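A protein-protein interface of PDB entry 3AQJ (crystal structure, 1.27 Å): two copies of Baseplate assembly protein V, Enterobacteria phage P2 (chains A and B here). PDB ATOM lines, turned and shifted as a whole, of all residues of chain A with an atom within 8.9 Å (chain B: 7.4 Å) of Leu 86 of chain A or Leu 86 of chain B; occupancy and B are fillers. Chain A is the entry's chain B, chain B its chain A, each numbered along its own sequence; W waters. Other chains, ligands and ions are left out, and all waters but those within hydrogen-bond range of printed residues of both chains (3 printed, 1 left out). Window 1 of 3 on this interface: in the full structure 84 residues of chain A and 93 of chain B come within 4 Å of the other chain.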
ATOM      1  N   VAL A  73     -32.945   2.669 -22.814  1.00  0.00           N
ATOM      2  CA  VAL A  73     -31.822   1.737 -23.130  1.00  0.00           C
ATOM      3  C   VAL A  73     -30.902   1.764 -21.937  1.00  0.00           C
ATOM      4  O   VAL A  73     -30.376   2.864 -21.614  1.00  0.00           O
ATOM      5  CB  VAL A  73     -31.081   2.176 -24.405  1.00  0.00           C
ATOM      6  CG1 VAL A  73     -29.852   1.247 -24.648  1.00  0.00           C
ATOM      7  CG2 VAL A  73     -31.998   2.170 -25.597  1.00  0.00           C
ATOM      8  N   LEU A  75     -27.306   0.325 -20.391  1.00  0.00           N
ATOM      9  CA  LEU A  75     -26.026  -0.319 -20.586  1.00  0.00           C
ATOM     10  C   LEU A  75     -25.480  -0.539 -19.168  1.00  0.00           C
ATOM     11  O   LEU A  75     -24.880   0.356 -18.541  1.00  0.00           O
ATOM     12  CB  LEU A  75     -25.159   0.561 -21.442  1.00  0.00           C
ATOM     13  CG  LEU A  75     -25.769   0.957 -22.801  1.00  0.00           C
ATOM     14  CD1 LEU A  75     -24.790   1.894 -23.570  1.00  0.00           C
ATOM     15  CD2 LEU A  75     -26.228  -0.249 -23.628  1.00  0.00           C
ATOM     16  N   VAL A  80     -18.819   1.674 -20.654  1.00  0.00           N
ATOM     17  CA  VAL A  80     -19.277   1.860 -22.031  1.00  0.00           C
ATOM     18  C   VAL A  80     -18.179   2.670 -22.709  1.00  0.00           C
ATOM     19  O   VAL A  80     -17.853   3.739 -22.206  1.00  0.00           O
ATOM     20  CB  VAL A  80     -20.604   2.617 -22.102  1.00  0.00           C
ATOM     21  CG1 VAL A  80     -20.987   2.928 -23.569  1.00  0.00           C
ATOM     22  CG2 VAL A  80     -21.743   1.804 -21.372  1.00  0.00           C
ATOM     23  N   VAL A  81     -17.661   2.211 -23.819  1.00  0.00           N
ATOM     24  CA  VAL A  81     -16.609   2.942 -24.590  1.00  0.00           C
ATOM     25  C   VAL A  81     -17.131   3.337 -25.908  1.00  0.00           C
ATOM     26  O   VAL A  81     -17.527   2.448 -26.733  1.00  0.00           O
ATOM     27  CB  VAL A  81     -15.371   2.049 -24.765  1.00  0.00           C
ATOM     28  CG1 VAL A  81     -14.261   2.764 -25.607  1.00  0.00           C
ATOM     29  CG2 VAL A  81     -14.812   1.629 -23.407  1.00  0.00           C
ATOM     30  N   CYS A  82     -17.189   4.644 -26.196  1.00  0.00           N
ATOM     31  CA  CYS A  82     -17.529   5.117 -27.523  1.00  0.00           C
ATOM     32  C   CYS A  82     -16.225   5.517 -28.154  1.00  0.00           C
ATOM     33  O   CYS A  82     -15.498   6.353 -27.577  1.00  0.00           O
ATOM     34  CB  CYS A  82     -18.426   6.350 -27.457  1.00  0.00           C
ATOM     35  SG  CYS A  82     -19.977   6.043 -26.545  1.00  0.00           S
ATOM     36  N   THR A  83     -15.859   4.904 -29.275  1.00  0.00           N
ATOM     37  CA  THR A  83     -14.494   5.053 -29.793  1.00  0.00           C
ATOM     38  C   THR A  83     -14.217   6.421 -30.393  1.00  0.00           C
ATOM     39  O   THR A  83     -13.031   6.764 -30.570  1.00  0.00           O
ATOM     40  CB  THR A  83     -14.166   3.941 -30.787  1.00  0.00           C
ATOM     41  OG1 THR A  83     -15.136   4.001 -31.785  1.00  0.00           O
ATOM     42  CG2 THR A  83     -14.145   2.605 -30.087  1.00  0.00           C
ATOM     43  N   ASN A  84     -15.221   7.131 -30.796  1.00  0.00           N
ATOM     44  CA  ASN A  84     -15.070   8.449 -31.502  1.00  0.00           C
ATOM     45  C   ASN A  84     -16.038   9.460 -30.904  1.00  0.00           C
ATOM     46  O   ASN A  84     -15.833   9.821 -29.697  1.00  0.00           O
ATOM     47  CB  ASN A  84     -15.216   8.316 -33.011  1.00  0.00           C
ATOM     48  CG  ASN A  84     -14.125   7.445 -33.580  1.00  0.00           C
ATOM     49  OD1 ASN A  84     -13.016   7.970 -33.852  1.00  0.00           O
ATOM     50  ND2 ASN A  84     -14.352   6.124 -33.702  1.00  0.00           N
ATOM     51  N   ARG A  85     -17.026   9.908 -31.636  1.00  0.00           N
ATOM     52  CA  ARG A  85     -17.931  10.947 -31.165  1.00  0.00           C
ATOM     53  C   ARG A  85     -19.112  10.345 -30.446  1.00  0.00           C
ATOM     54  O   ARG A  85     -19.701   9.350 -30.886  1.00  0.00           O
ATOM     55  CB  ARG A  85     -18.500  11.722 -32.363  1.00  0.00           C
ATOM     56  CG  ARG A  85     -19.113  13.048 -31.959  1.00  0.00           C
ATOM     57  CD  ARG A  85     -19.711  13.787 -33.114  1.00  0.00           C
ATOM     58  NE  ARG A  85     -18.750  14.374 -34.024  1.00  0.00           N
ATOM     59  CZ  ARG A  85     -17.951  15.390 -33.701  1.00  0.00           C
ATOM     60  NH1 ARG A  85     -17.959  15.912 -32.453  1.00  0.00           N
ATOM     61  NH2 ARG A  85     -17.141  15.905 -34.608  1.00  0.00           N
ATOM     62  N   LEU A  86     -19.518  11.051 -29.379  1.00  0.00           N
ATOM     63  CA  LEU A  86     -20.772  10.782 -28.660  1.00  0.00           C
ATOM     64  C   LEU A  86     -21.608  12.040 -28.698  1.00  0.00           C
ATOM     65  O   LEU A  86     -21.067  13.101 -28.266  1.00  0.00           O
ATOM     66  CB  LEU A  86     -20.413  10.399 -27.210  1.00  0.00           C
ATOM     67  CG  LEU A  86     -21.650  10.277 -26.294  1.00  0.00           C
ATOM     68  CD1 LEU A  86     -22.669   9.255 -26.733  1.00  0.00           C
ATOM     69  CD2 LEU A  86     -21.100   9.997 -24.950  1.00  0.00           C
ATOM     70  N   ILE A  87     -22.829  11.978 -29.229  1.00  0.00           N
ATOM     71  CA  ILE A  87     -23.709  13.133 -29.337  1.00  0.00           C
ATOM     72  C   ILE A  87     -24.906  12.809 -28.491  1.00  0.00           C
ATOM     73  O   ILE A  87     -25.493  11.694 -28.595  1.00  0.00           O
ATOM     74  CB  ILE A  87     -24.198  13.329 -30.792  1.00  0.00           C
ATOM     75  CG1 ILE A  87     -22.978  13.541 -31.682  1.00  0.00           C
ATOM     76  CG2 ILE A  87     -25.163  14.459 -30.936  1.00  0.00           C
ATOM     77  CD1 ILE A  87     -23.423  13.786 -33.231  1.00  0.00           C
ATOM     78  N   THR A  88     -25.377  13.741 -27.653  1.00  0.00           N
ATOM     79  CA  THR A  88     -26.626  13.550 -26.900  1.00  0.00           C
ATOM     80  C   THR A  88     -27.395  14.841 -26.839  1.00  0.00           C
ATOM     81  O   THR A  88     -26.847  15.929 -26.976  1.00  0.00           O
ATOM     82  CB  THR A  88     -26.364  13.044 -25.464  1.00  0.00           C
ATOM     83  OG1 THR A  88     -27.624  12.792 -24.827  1.00  0.00           O
ATOM     84  CG2 THR A  88     -25.502  14.063 -24.623  1.00  0.00           C
ATOM     85  N   GLY A  89     -28.669  14.686 -26.651  1.00  0.00           N
ATOM     86  CA  GLY A  89     -29.551  15.867 -26.398  1.00  0.00           C
ATOM     87  C   GLY A  89     -29.200  16.491 -25.076  1.00  0.00           C
ATOM     88  O   GLY A  89     -28.776  17.669 -25.035  1.00  0.00           O
ATOM     89  N   THR A  90     -29.401  15.791 -24.007  1.00  0.00           N
ATOM     90  CA  THR A  90     -28.979  16.305 -22.691  1.00  0.00           C
ATOM     91  C   THR A  90     -28.082  15.235 -22.037  1.00  0.00           C
ATOM     92  O   THR A  90     -28.115  14.051 -22.386  1.00  0.00           O
ATOM     93  CB  THR A  90     -30.179  16.636 -21.797  1.00  0.00           C
ATOM     94  OG1 THR A  90     -30.952  15.432 -21.548  1.00  0.00           O
ATOM     95  CG2 THR A  90     -30.969  17.802 -22.454  1.00  0.00           C
ATOM     96  N   LEU A  91     -27.299  15.709 -21.098  1.00  0.00           N
ATOM     97  CA  LEU A  91     -26.356  14.854 -20.379  1.00  0.00           C
ATOM     98  C   LEU A  91     -26.589  14.932 -18.905  1.00  0.00           C
ATOM     99  O   LEU A  91     -26.723  16.084 -18.370  1.00  0.00           O
ATOM    100  CB  LEU A  91     -24.914  15.312 -20.743  1.00  0.00           C
ATOM    101  CG  LEU A  91     -23.836  14.577 -19.950  1.00  0.00           C
ATOM    102  CD1 LEU A  91     -23.728  13.103 -20.383  1.00  0.00           C
ATOM    103  CD2 LEU A  91     -22.502  15.428 -20.172  1.00  0.00           C
ATOM    104  N   GLU A  92     -26.523  13.826 -18.200  1.00  0.00           N
ATOM    105  CA  GLU A  92     -26.531  13.856 -16.738  1.00  0.00           C
ATOM    106  C   GLU A  92     -25.405  12.988 -16.247  1.00  0.00           C
ATOM    107  O   GLU A  92     -25.315  11.772 -16.588  1.00  0.00           O
ATOM    108  CB  GLU A  92     -27.867  13.263 -16.256  1.00  0.00           C
ATOM    109  CG  GLU A  92     -27.989  13.195 -14.741  1.00  0.00           C
ATOM    110  CD  GLU A  92     -29.301  12.518 -14.268  1.00  0.00           C
ATOM    111  OE1 GLU A  92     -30.244  12.422 -15.088  1.00  0.00           O
ATOM    112  OE2 GLU A  92     -29.247  12.056 -13.077  1.00  0.00           O
ATOM    113  N   VAL A  93     -24.502  13.560 -15.469  1.00  0.00           N
ATOM    114  CA  VAL A  93     -23.372  12.870 -14.884  1.00  0.00           C
ATOM    115  C   VAL A  93     -23.627  12.784 -13.395  1.00  0.00           C
ATOM    116  O   VAL A  93     -23.798  13.852 -12.771  1.00  0.00           O
ATOM    117  CB  VAL A  93     -22.034  13.575 -15.157  1.00  0.00           C
ATOM    118  CG1 VAL A  93     -20.878  12.852 -14.486  1.00  0.00           C
ATOM    119  CG2 VAL A  93     -21.809  13.699 -16.648  1.00  0.00           C
ATOM    120  N   GLN A  94     -23.650  11.607 -12.835  1.00  0.00           N
ATOM    121  CA  GLN A  94     -24.152  11.487 -11.446  1.00  0.00           C
ATOM    122  C   GLN A  94     -23.048  11.550 -10.413  1.00  0.00           C
ATOM    123  O   GLN A  94     -23.339  12.064  -9.282  1.00  0.00           O
ATOM    124  CB  GLN A  94     -24.868  10.117 -11.285  1.00  0.00           C
ATOM    125  CG  GLN A  94     -26.078   9.961 -12.163  1.00  0.00           C
ATOM    126  CD  GLN A  94     -26.607   8.552 -12.171  1.00  0.00           C
ATOM    127  OE1 GLN A  94     -25.871   7.604 -12.276  1.00  0.00           O
ATOM    128  NE2 GLN A  94     -27.935   8.429 -12.107  1.00  0.00           N
ATOM    129  N   LEU B  75     -18.857   0.644 -28.311  1.00  0.00           N
ATOM    130  CA  LEU B  75     -19.553   1.145 -29.512  1.00  0.00           C
ATOM    131  C   LEU B  75     -18.451   1.726 -30.406  1.00  0.00           C
ATOM    132  O   LEU B  75     -17.983   2.853 -30.207  1.00  0.00           O
ATOM    133  CB  LEU B  75     -20.560   2.160 -29.057  1.00  0.00           C
ATOM    134  CG  LEU B  75     -21.589   1.656 -27.996  1.00  0.00           C
ATOM    135  CD1 LEU B  75     -22.563   2.803 -27.583  1.00  0.00           C
ATOM    136  CD2 LEU B  75     -22.349   0.409 -28.489  1.00  0.00           C
ATOM    137  N   THR B  77     -17.711   3.090 -33.469  1.00  0.00           N
ATOM    138  CA  THR B  77     -18.450   3.773 -34.520  1.00  0.00           C
ATOM    139  C   THR B  77     -17.951   5.209 -34.573  1.00  0.00           C
ATOM    140  O   THR B  77     -17.529   5.783 -33.561  1.00  0.00           O
ATOM    141  CB  THR B  77     -19.950   3.767 -34.210  1.00  0.00           C
ATOM    142  OG1 THR B  77     -20.735   4.440 -35.184  1.00  0.00           O
ATOM    143  CG2 THR B  77     -20.283   4.390 -32.840  1.00  0.00           C
ATOM    144  N   PRO B  78     -18.072   5.866 -35.752  1.00  0.00           N
ATOM    145  CA  PRO B  78     -17.665   7.283 -35.760  1.00  0.00           C
ATOM    146  C   PRO B  78     -18.640   8.087 -34.910  1.00  0.00           C
ATOM    147  O   PRO B  78     -18.172   9.133 -34.373  1.00  0.00           O
ATOM    148  CB  PRO B  78     -17.805   7.629 -37.266  1.00  0.00           C
ATOM    149  CG  PRO B  78     -17.468   6.333 -38.004  1.00  0.00           C
ATOM    150  CD  PRO B  78     -18.212   5.297 -37.124  1.00  0.00           C
ATOM    151  N   GLU B  79     -19.876   7.659 -34.722  1.00  0.00           N
ATOM    152  CA  GLU B  79     -20.809   8.499 -33.922  1.00  0.00           C
ATOM    153  C   GLU B  79     -21.834   7.631 -33.240  1.00  0.00           C
ATOM    154  O   GLU B  79     -22.543   6.826 -33.879  1.00  0.00           O
ATOM    155  CB  GLU B  79     -21.492   9.462 -34.870  1.00  0.00           C
ATOM    156  CG  GLU B  79     -22.237  10.649 -34.355  1.00  0.00           C
ATOM    157  CD  GLU B  79     -22.632  11.578 -35.540  1.00  0.00           C
ATOM    158  OE1 GLU B  79     -21.811  12.406 -36.098  1.00  0.00           O
ATOM    159  OE2 GLU B  79     -23.785  11.442 -35.940  1.00  0.00           O
ATOM    160  N   VAL B  80     -21.966   7.886 -31.945  1.00  0.00           N
ATOM    161  CA  VAL B  80     -23.082   7.350 -31.152  1.00  0.00           C
ATOM    162  C   VAL B  80     -24.019   8.535 -30.974  1.00  0.00           C
ATOM    163  O   VAL B  80     -23.515   9.587 -30.504  1.00  0.00           O
ATOM    164  CB  VAL B  80     -22.584   6.799 -29.804  1.00  0.00           C
ATOM    165  CG1 VAL B  80     -23.750   6.363 -28.883  1.00  0.00           C
ATOM    166  CG2 VAL B  80     -21.604   5.672 -30.011  1.00  0.00           C
ATOM    167  N   VAL B  81     -25.301   8.400 -31.232  1.00  0.00           N
ATOM    168  CA  VAL B  81     -26.270   9.437 -31.008  1.00  0.00           C
ATOM    169  C   VAL B  81     -27.306   8.983 -30.054  1.00  0.00           C
ATOM    170  O   VAL B  81     -27.988   7.972 -30.338  1.00  0.00           O
ATOM    171  CB  VAL B  81     -26.946   9.850 -32.344  1.00  0.00           C
ATOM    172  CG1 VAL B  81     -28.062  10.871 -32.109  1.00  0.00           C
ATOM    173  CG2 VAL B  81     -25.895  10.342 -33.313  1.00  0.00           C
ATOM    174  N   CYS B  82     -27.477   9.729 -28.956  1.00  0.00           N
ATOM    175  CA  CYS B  82     -28.572   9.514 -28.031  1.00  0.00           C
ATOM    176  C   CYS B  82     -29.567  10.631 -28.315  1.00  0.00           C
ATOM    177  O   CYS B  82     -29.183  11.826 -28.223  1.00  0.00           O
ATOM    178  CB  CYS B  82     -28.078   9.586 -26.585  1.00  0.00           C
ATOM    179  SG  CYS B  82     -26.770   8.399 -26.228  1.00  0.00           S
ATOM    180  N   THR B  83     -30.798  10.338 -28.648  1.00  0.00           N
ATOM    181  CA  THR B  83     -31.687  11.375 -29.194  1.00  0.00           C
ATOM    182  C   THR B  83     -32.201  12.250 -28.034  1.00  0.00           C
ATOM    183  O   THR B  83     -32.787  13.329 -28.375  1.00  0.00           O
ATOM    184  CB  THR B  83     -32.868  10.705 -29.910  1.00  0.00           C
ATOM    185  OG1 THR B  83     -33.538   9.841 -29.027  1.00  0.00           O
ATOM    186  CG2 THR B  83     -32.300  10.017 -31.168  1.00  0.00           C
ATOM    187  N   ASN B  84     -32.218  11.849 -26.779  1.00  0.00           N
ATOM    188  CA  ASN B  84     -32.733  12.624 -25.660  1.00  0.00           C
ATOM    189  C   ASN B  84     -31.706  12.653 -24.544  1.00  0.00           C
ATOM    190  O   ASN B  84     -30.646  13.292 -24.796  1.00  0.00           O
ATOM    191  CB  ASN B  84     -34.159  12.136 -25.237  1.00  0.00           C
ATOM    192  CG  ASN B  84     -35.148  12.376 -26.344  1.00  0.00           C
ATOM    193  OD1 ASN B  84     -35.757  13.471 -26.426  1.00  0.00           O
ATOM    194  ND2 ASN B  84     -35.333  11.384 -27.179  1.00  0.00           N
ATOM    195  N   ARG B  85     -31.984  12.066 -23.441  1.00  0.00           N
ATOM    196  CA  ARG B  85     -31.084  12.170 -22.296  1.00  0.00           C
ATOM    197  C   ARG B  85     -30.162  11.001 -22.272  1.00  0.00           C
ATOM    198  O   ARG B  85     -30.496   9.820 -22.648  1.00  0.00           O
ATOM    199  CB  ARG B  85     -31.877  12.092 -20.993  1.00  0.00           C
ATOM    200  CG  ARG B  85     -31.030  12.714 -19.853  1.00  0.00           C
ATOM    201  CD  ARG B  85     -31.889  13.305 -18.736  1.00  0.00           C
ATOM    202  NE  ARG B  85     -32.944  12.355 -18.483  1.00  0.00           N
ATOM    203  CZ  ARG B  85     -34.209  12.654 -18.189  1.00  0.00           C
ATOM    204  NH1 ARG B  85     -34.618  13.931 -18.062  1.00  0.00           N
ATOM    205  NH2 ARG B  85     -35.034  11.631 -18.001  1.00  0.00           N
ATOM    206  N   LEU B  86     -28.914  11.262 -21.908  1.00  0.00           N
ATOM    207  CA  LEU B  86     -27.868  10.282 -21.645  1.00  0.00           C
ATOM    208  C   LEU B  86     -27.457  10.453 -20.184  1.00  0.00           C
ATOM    209  O   LEU B  86     -27.116  11.592 -19.766  1.00  0.00           O
ATOM    210  CB  LEU B  86     -26.671  10.583 -22.526  1.00  0.00           C
ATOM    211  CG  LEU B  86     -25.457   9.757 -22.145  1.00  0.00           C
ATOM    212  CD1 LEU B  86     -25.668   8.311 -22.251  1.00  0.00           C
ATOM    213  CD2 LEU B  86     -24.329  10.186 -23.161  1.00  0.00           C
ATOM    214  N   ILE B  87     -27.571   9.444 -19.346  1.00  0.00           N
ATOM    215  CA  ILE B  87     -27.258   9.452 -17.912  1.00  0.00           C
ATOM    216  C   ILE B  87     -26.115   8.520 -17.716  1.00  0.00           C
ATOM    217  O   ILE B  87     -26.136   7.378 -18.239  1.00  0.00           O
ATOM    218  CB  ILE B  87     -28.466   8.941 -17.046  1.00  0.00           C
ATOM    219  CG1 ILE B  87     -29.684   9.799 -17.405  1.00  0.00           C
ATOM    220  CG2 ILE B  87     -28.128   8.906 -15.573  1.00  0.00           C
ATOM    221  CD1 ILE B  87     -31.017   9.354 -16.706  1.00  0.00           C
ATOM    222  N   THR B  88     -25.085   8.899 -16.987  1.00  0.00           N
ATOM    223  CA  THR B  88     -24.018   7.994 -16.650  1.00  0.00           C
ATOM    224  C   THR B  88     -23.595   8.189 -15.177  1.00  0.00           C
ATOM    225  O   THR B  88     -23.781   9.311 -14.586  1.00  0.00           O
ATOM    226  CB  THR B  88     -22.827   8.201 -17.605  1.00  0.00           C
ATOM    227  OG1 THR B  88     -21.889   7.186 -17.331  1.00  0.00           O
ATOM    228  CG2 THR B  88     -22.118   9.603 -17.475  1.00  0.00           C
ATOM    229  N   LEU B  91     -18.114  10.070 -16.103  1.00  0.00           N
ATOM    230  CA  LEU B  91     -17.807  10.425 -17.524  1.00  0.00           C
ATOM    231  C   LEU B  91     -16.304  10.564 -17.749  1.00  0.00           C
ATOM    232  O   LEU B  91     -15.675  11.218 -16.872  1.00  0.00           O
ATOM    233  CB  LEU B  91     -18.545  11.714 -17.852  1.00  0.00           C
ATOM    234  CG  LEU B  91     -18.243  12.251 -19.238  1.00  0.00           C
ATOM    235  CD1 LEU B  91     -18.799  11.366 -20.305  1.00  0.00           C
ATOM    236  CD2 LEU B  91     -18.785  13.679 -19.305  1.00  0.00           C
ATOM    237  N   GLU B  92     -15.767  10.020 -18.827  1.00  0.00           N
ATOM    238  CA  GLU B  92     -14.404  10.309 -19.199  1.00  0.00           C
ATOM    239  C   GLU B  92     -14.423  10.778 -20.614  1.00  0.00           C
ATOM    240  O   GLU B  92     -14.756  10.031 -21.544  1.00  0.00           O
ATOM    241  CB  GLU B  92     -13.520   9.077 -19.029  1.00  0.00           C
ATOM    242  CG  GLU B  92     -13.400   8.764 -17.523  1.00  0.00           C
ATOM    243  CD  GLU B  92     -13.036   7.280 -17.363  1.00  0.00           C
ATOM    244  OE1 GLU B  92     -11.929   6.917 -17.868  1.00  0.00           O
ATOM    245  OE2 GLU B  92     -13.863   6.499 -16.778  1.00  0.00           O
ATOM    246  N   VAL B  93     -14.082  12.031 -20.870  1.00  0.00           N
ATOM    247  CA  VAL B  93     -13.946  12.569 -22.239  1.00  0.00           C
ATOM    248  C   VAL B  93     -12.458  12.655 -22.584  1.00  0.00           C
ATOM    249  O   VAL B  93     -11.699  13.267 -21.800  1.00  0.00           O
ATOM    250  CB  VAL B  93     -14.565  13.979 -22.346  1.00  0.00           C
ATOM    251  CG1 VAL B  93     -14.416  14.501 -23.746  1.00  0.00           C
ATOM    252  CG2 VAL B  93     -16.021  13.928 -22.009  1.00  0.00           C
ATOM    253  N   THR B  98     -17.786  19.692 -27.359  1.00  0.00           N
ATOM    254  CA  THR B  98     -18.556  20.902 -27.339  1.00  0.00           C
ATOM    255  C   THR B  98     -19.787  20.642 -26.486  1.00  0.00           C
ATOM    256  O   THR B  98     -20.323  19.492 -26.348  1.00  0.00           O
ATOM    257  CB  THR B  98     -19.008  21.314 -28.731  1.00  0.00           C
ATOM    258  OG1 THR B  98     -19.847  20.318 -29.327  1.00  0.00           O
ATOM    259  CG2 THR B  98     -17.867  21.649 -29.590  1.00  0.00           C
HETATM  260  O   HOH W   1     -33.034  15.228 -23.353  1.00  0.00           O
HETATM  261  O   HOH W   2     -18.098   6.844 -30.993  1.00  0.00           O
HETATM  262  O   HOH W   3     -19.053  18.935 -31.833  1.00  0.00           O
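CA of Glu 79 of chain B touches O of Arg 85 of chain A (3.3 Å). Val 80 of chain B touches Leu 86 of chain A. Ile 87 of chain A touches Glu 79 of chain B (CD1 to CD, 3.3 Å). Val 81 of chain B touches Ile 87 of chain A. Cys 82 of chain B touches Thr 88 of chain A. Thr 88 of chain A touches Leu 86 of chain B. CG of Arg 85 of chain B touches OG1 of Thr 90 of chain A, 3.2 Å away. Leu 91 of chain A touches Leu 86 of chain B. Glu 92 of chain A touches Ile 87 of chain B. Thr 88 of chain B touches Val 93 of chain A.
The backbone NH of Leu 75 of chain B is in hydrogen-bond range of the backbone carbonyl oxygen of Val 81 of chain A, at 2.7 Å. N of Thr 83 of chain A is in hydrogen-bond range of O of Leu 75 of chain B (3.1 Å). The backbone NH of Thr 77 of chain B is in hydrogen-bond range of the side-chain hydroxyl of Thr 83 of chain A (3.2 Å). The backbone carbonyl oxygen (O) of Thr 77 of chain B sits at hydrogen-bond distance from the side-chain amide nitrogen (ND2) of Asn 84 of chain A, at 3.2 Å. The backbone carbonyl oxygen (O) of Pro 78 of chain B sits at hydrogen-bond distance from the backbone NH (N) of Arg 85 of chain A, at 3.1 Å. N of Val 80 of chain B sits at hydrogen-bond distance from O of Arg 85 of chain A, 2.9 Å away. O of Val 80 of chain B sits at hydrogen-bond distance from N of Ile 87 of chain A (2.8 Å). The backbone NH (N) of Cys 82 of chain B sits at hydrogen-bond distance from the backbone carbonyl oxygen (O) of Ile 87 of chain A (2.8 Å). N of Gly 89 of chain A sits at hydrogen-bond distance from O of Cys 82 of chain B (3.3 Å). O of Asn 84 of chain B is in hydrogen-bond range of OG1 of Thr 88 of chain A (3.1 Å). The backbone NH (N) of Gly 89 of chain A is in hydrogen-bond range of the backbone carbonyl oxygen (O) of Asn 84 of chain B, 3.0 Å away. N of Thr 90 of chain A lies within hydrogen-bond range of O of Asn 84 of chain B, at 2.9 Å. N of Leu 86 of chain B sits at hydrogen-bond distance from O of Thr 90 of chain A (2.9 Å). The backbone carbonyl oxygen of Leu 86 of chain B sits at hydrogen-bond distance from the backbone NH of Glu 92 of chain A (2.8 Å). The backbone NH (N) of Thr 88 of chain B is in hydrogen-bond range of the backbone carbonyl oxygen (O) of Glu 92 of chain A, at 2.9 Å. The backbone carbonyl oxygen (O) of Thr 88 of chain B lies within hydrogen-bond range of the backbone NH (N) of Gln 94 of chain A (2.9 Å).
Water W1 lies within hydrogen-bond range of OG1 of Thr 90 of chain A, N of Arg 85 of chain B and O of Asn 84 of chain B. Water W2 lies within hydrogen-bond range of O of Thr 77 of chain B (2.8 Å), N of Asn 84 of chain A (2.9 Å), O of Arg 85 of chain A (3.0 Å) and N of Thr 83 of chain A (3.4 Å). Water W3 bridges OG1 of Thr 98 of chain B (3.0 Å) and NH1 of Arg 85 of chain A (3.3 Å).
Thr 88 of chain A touches Cys 82 of chain B, but with the chains exchanged Cys 82 of chain A does not touch Thr 88 of chain B (9.5 Å). Thr 88 of chain A touches Asn 84 of chain B, but with the chains exchanged Asn 84 of chain A does not touch Thr 88 of chain B (13.7 Å). Leu 91 of chain A touches Leu 86 of chain B, but with the chains exchanged Leu 86 of chain A does not touch Leu 91 of chain B (5.4 Å). Glu 92 of chain A touches Thr 88 of chain B, but with the chains exchanged Thr 88 of chain A does not touch Glu 92 of chain B (11.9 Å). Of the 31 pairs that touch across the chains among the printed residues, 1 has its exchanged pair printed and touching as well.
Of the 17 printed residues of chain B, 12 touch a printed residue of chain A. Hydrophobic or aromatic side chains of chain B that line the printed part of chain A: Leu 75, Val 80, Leu 86 and Ile 87. Along chain B the printed residues that touch a printed residue of chain A span positions 75 to 88. Hydrophobic or aromatic side chains of chain A that line the printed part of chain B: Leu 86, Ile 87 and Leu 91. Along chain A the printed residues that touch a printed residue of chain B span positions 81 to 94. Among the printed residues, 31 pairs touch across the chains.
The backbone carbonyl oxygen (O) of Glu 79 of chain B is in hydrogen-bond range of the side-chain hydroxyl (OG1) of Thr 77 of chain B, 3.3 Å away. The side-chain hydroxyl of Thr 83 of chain B lies within hydrogen-bond range of the side-chain amide nitrogen of Asn 84 of chain B. The side-chain amide nitrogen of Asn 84 of chain A lies within hydrogen-bond range of the side-chain hydroxyl of Thr 83 of chain A (3.0 Å). O of Thr 90 of chain A is in hydrogen-bond range of OG1 of Thr 88 of chain A.
Leu 86 of chain B touches just these residues of chain A: Leu 86, Thr 88, Thr 90, Leu 91 and Glu 92. Of the printed residues of chain A, Thr 88 of chain B touches Glu 92 (2.9 Å), Val 93 (3.6 Å) and Gln 94 (2.9 Å). Printed residues of chain B within 4 Å of Ile 87 of chain A: Glu 79 (3.3 Å), Val 80 (2.8 Å), Val 81 (3.4 Å) and Cys 82 (2.8 Å). Of the printed residues of chain B, Asn 84 of chain A touches Thr 77 and Pro 78. Leu 75 of chain A touches none of the printed residues of chain B. Val 80 of chain A touches none of the printed residues of chain B. The nearest printed residue of chain B that does not touch Gly 89 of chain A is Thr 83 of chain B (4.5 Å).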
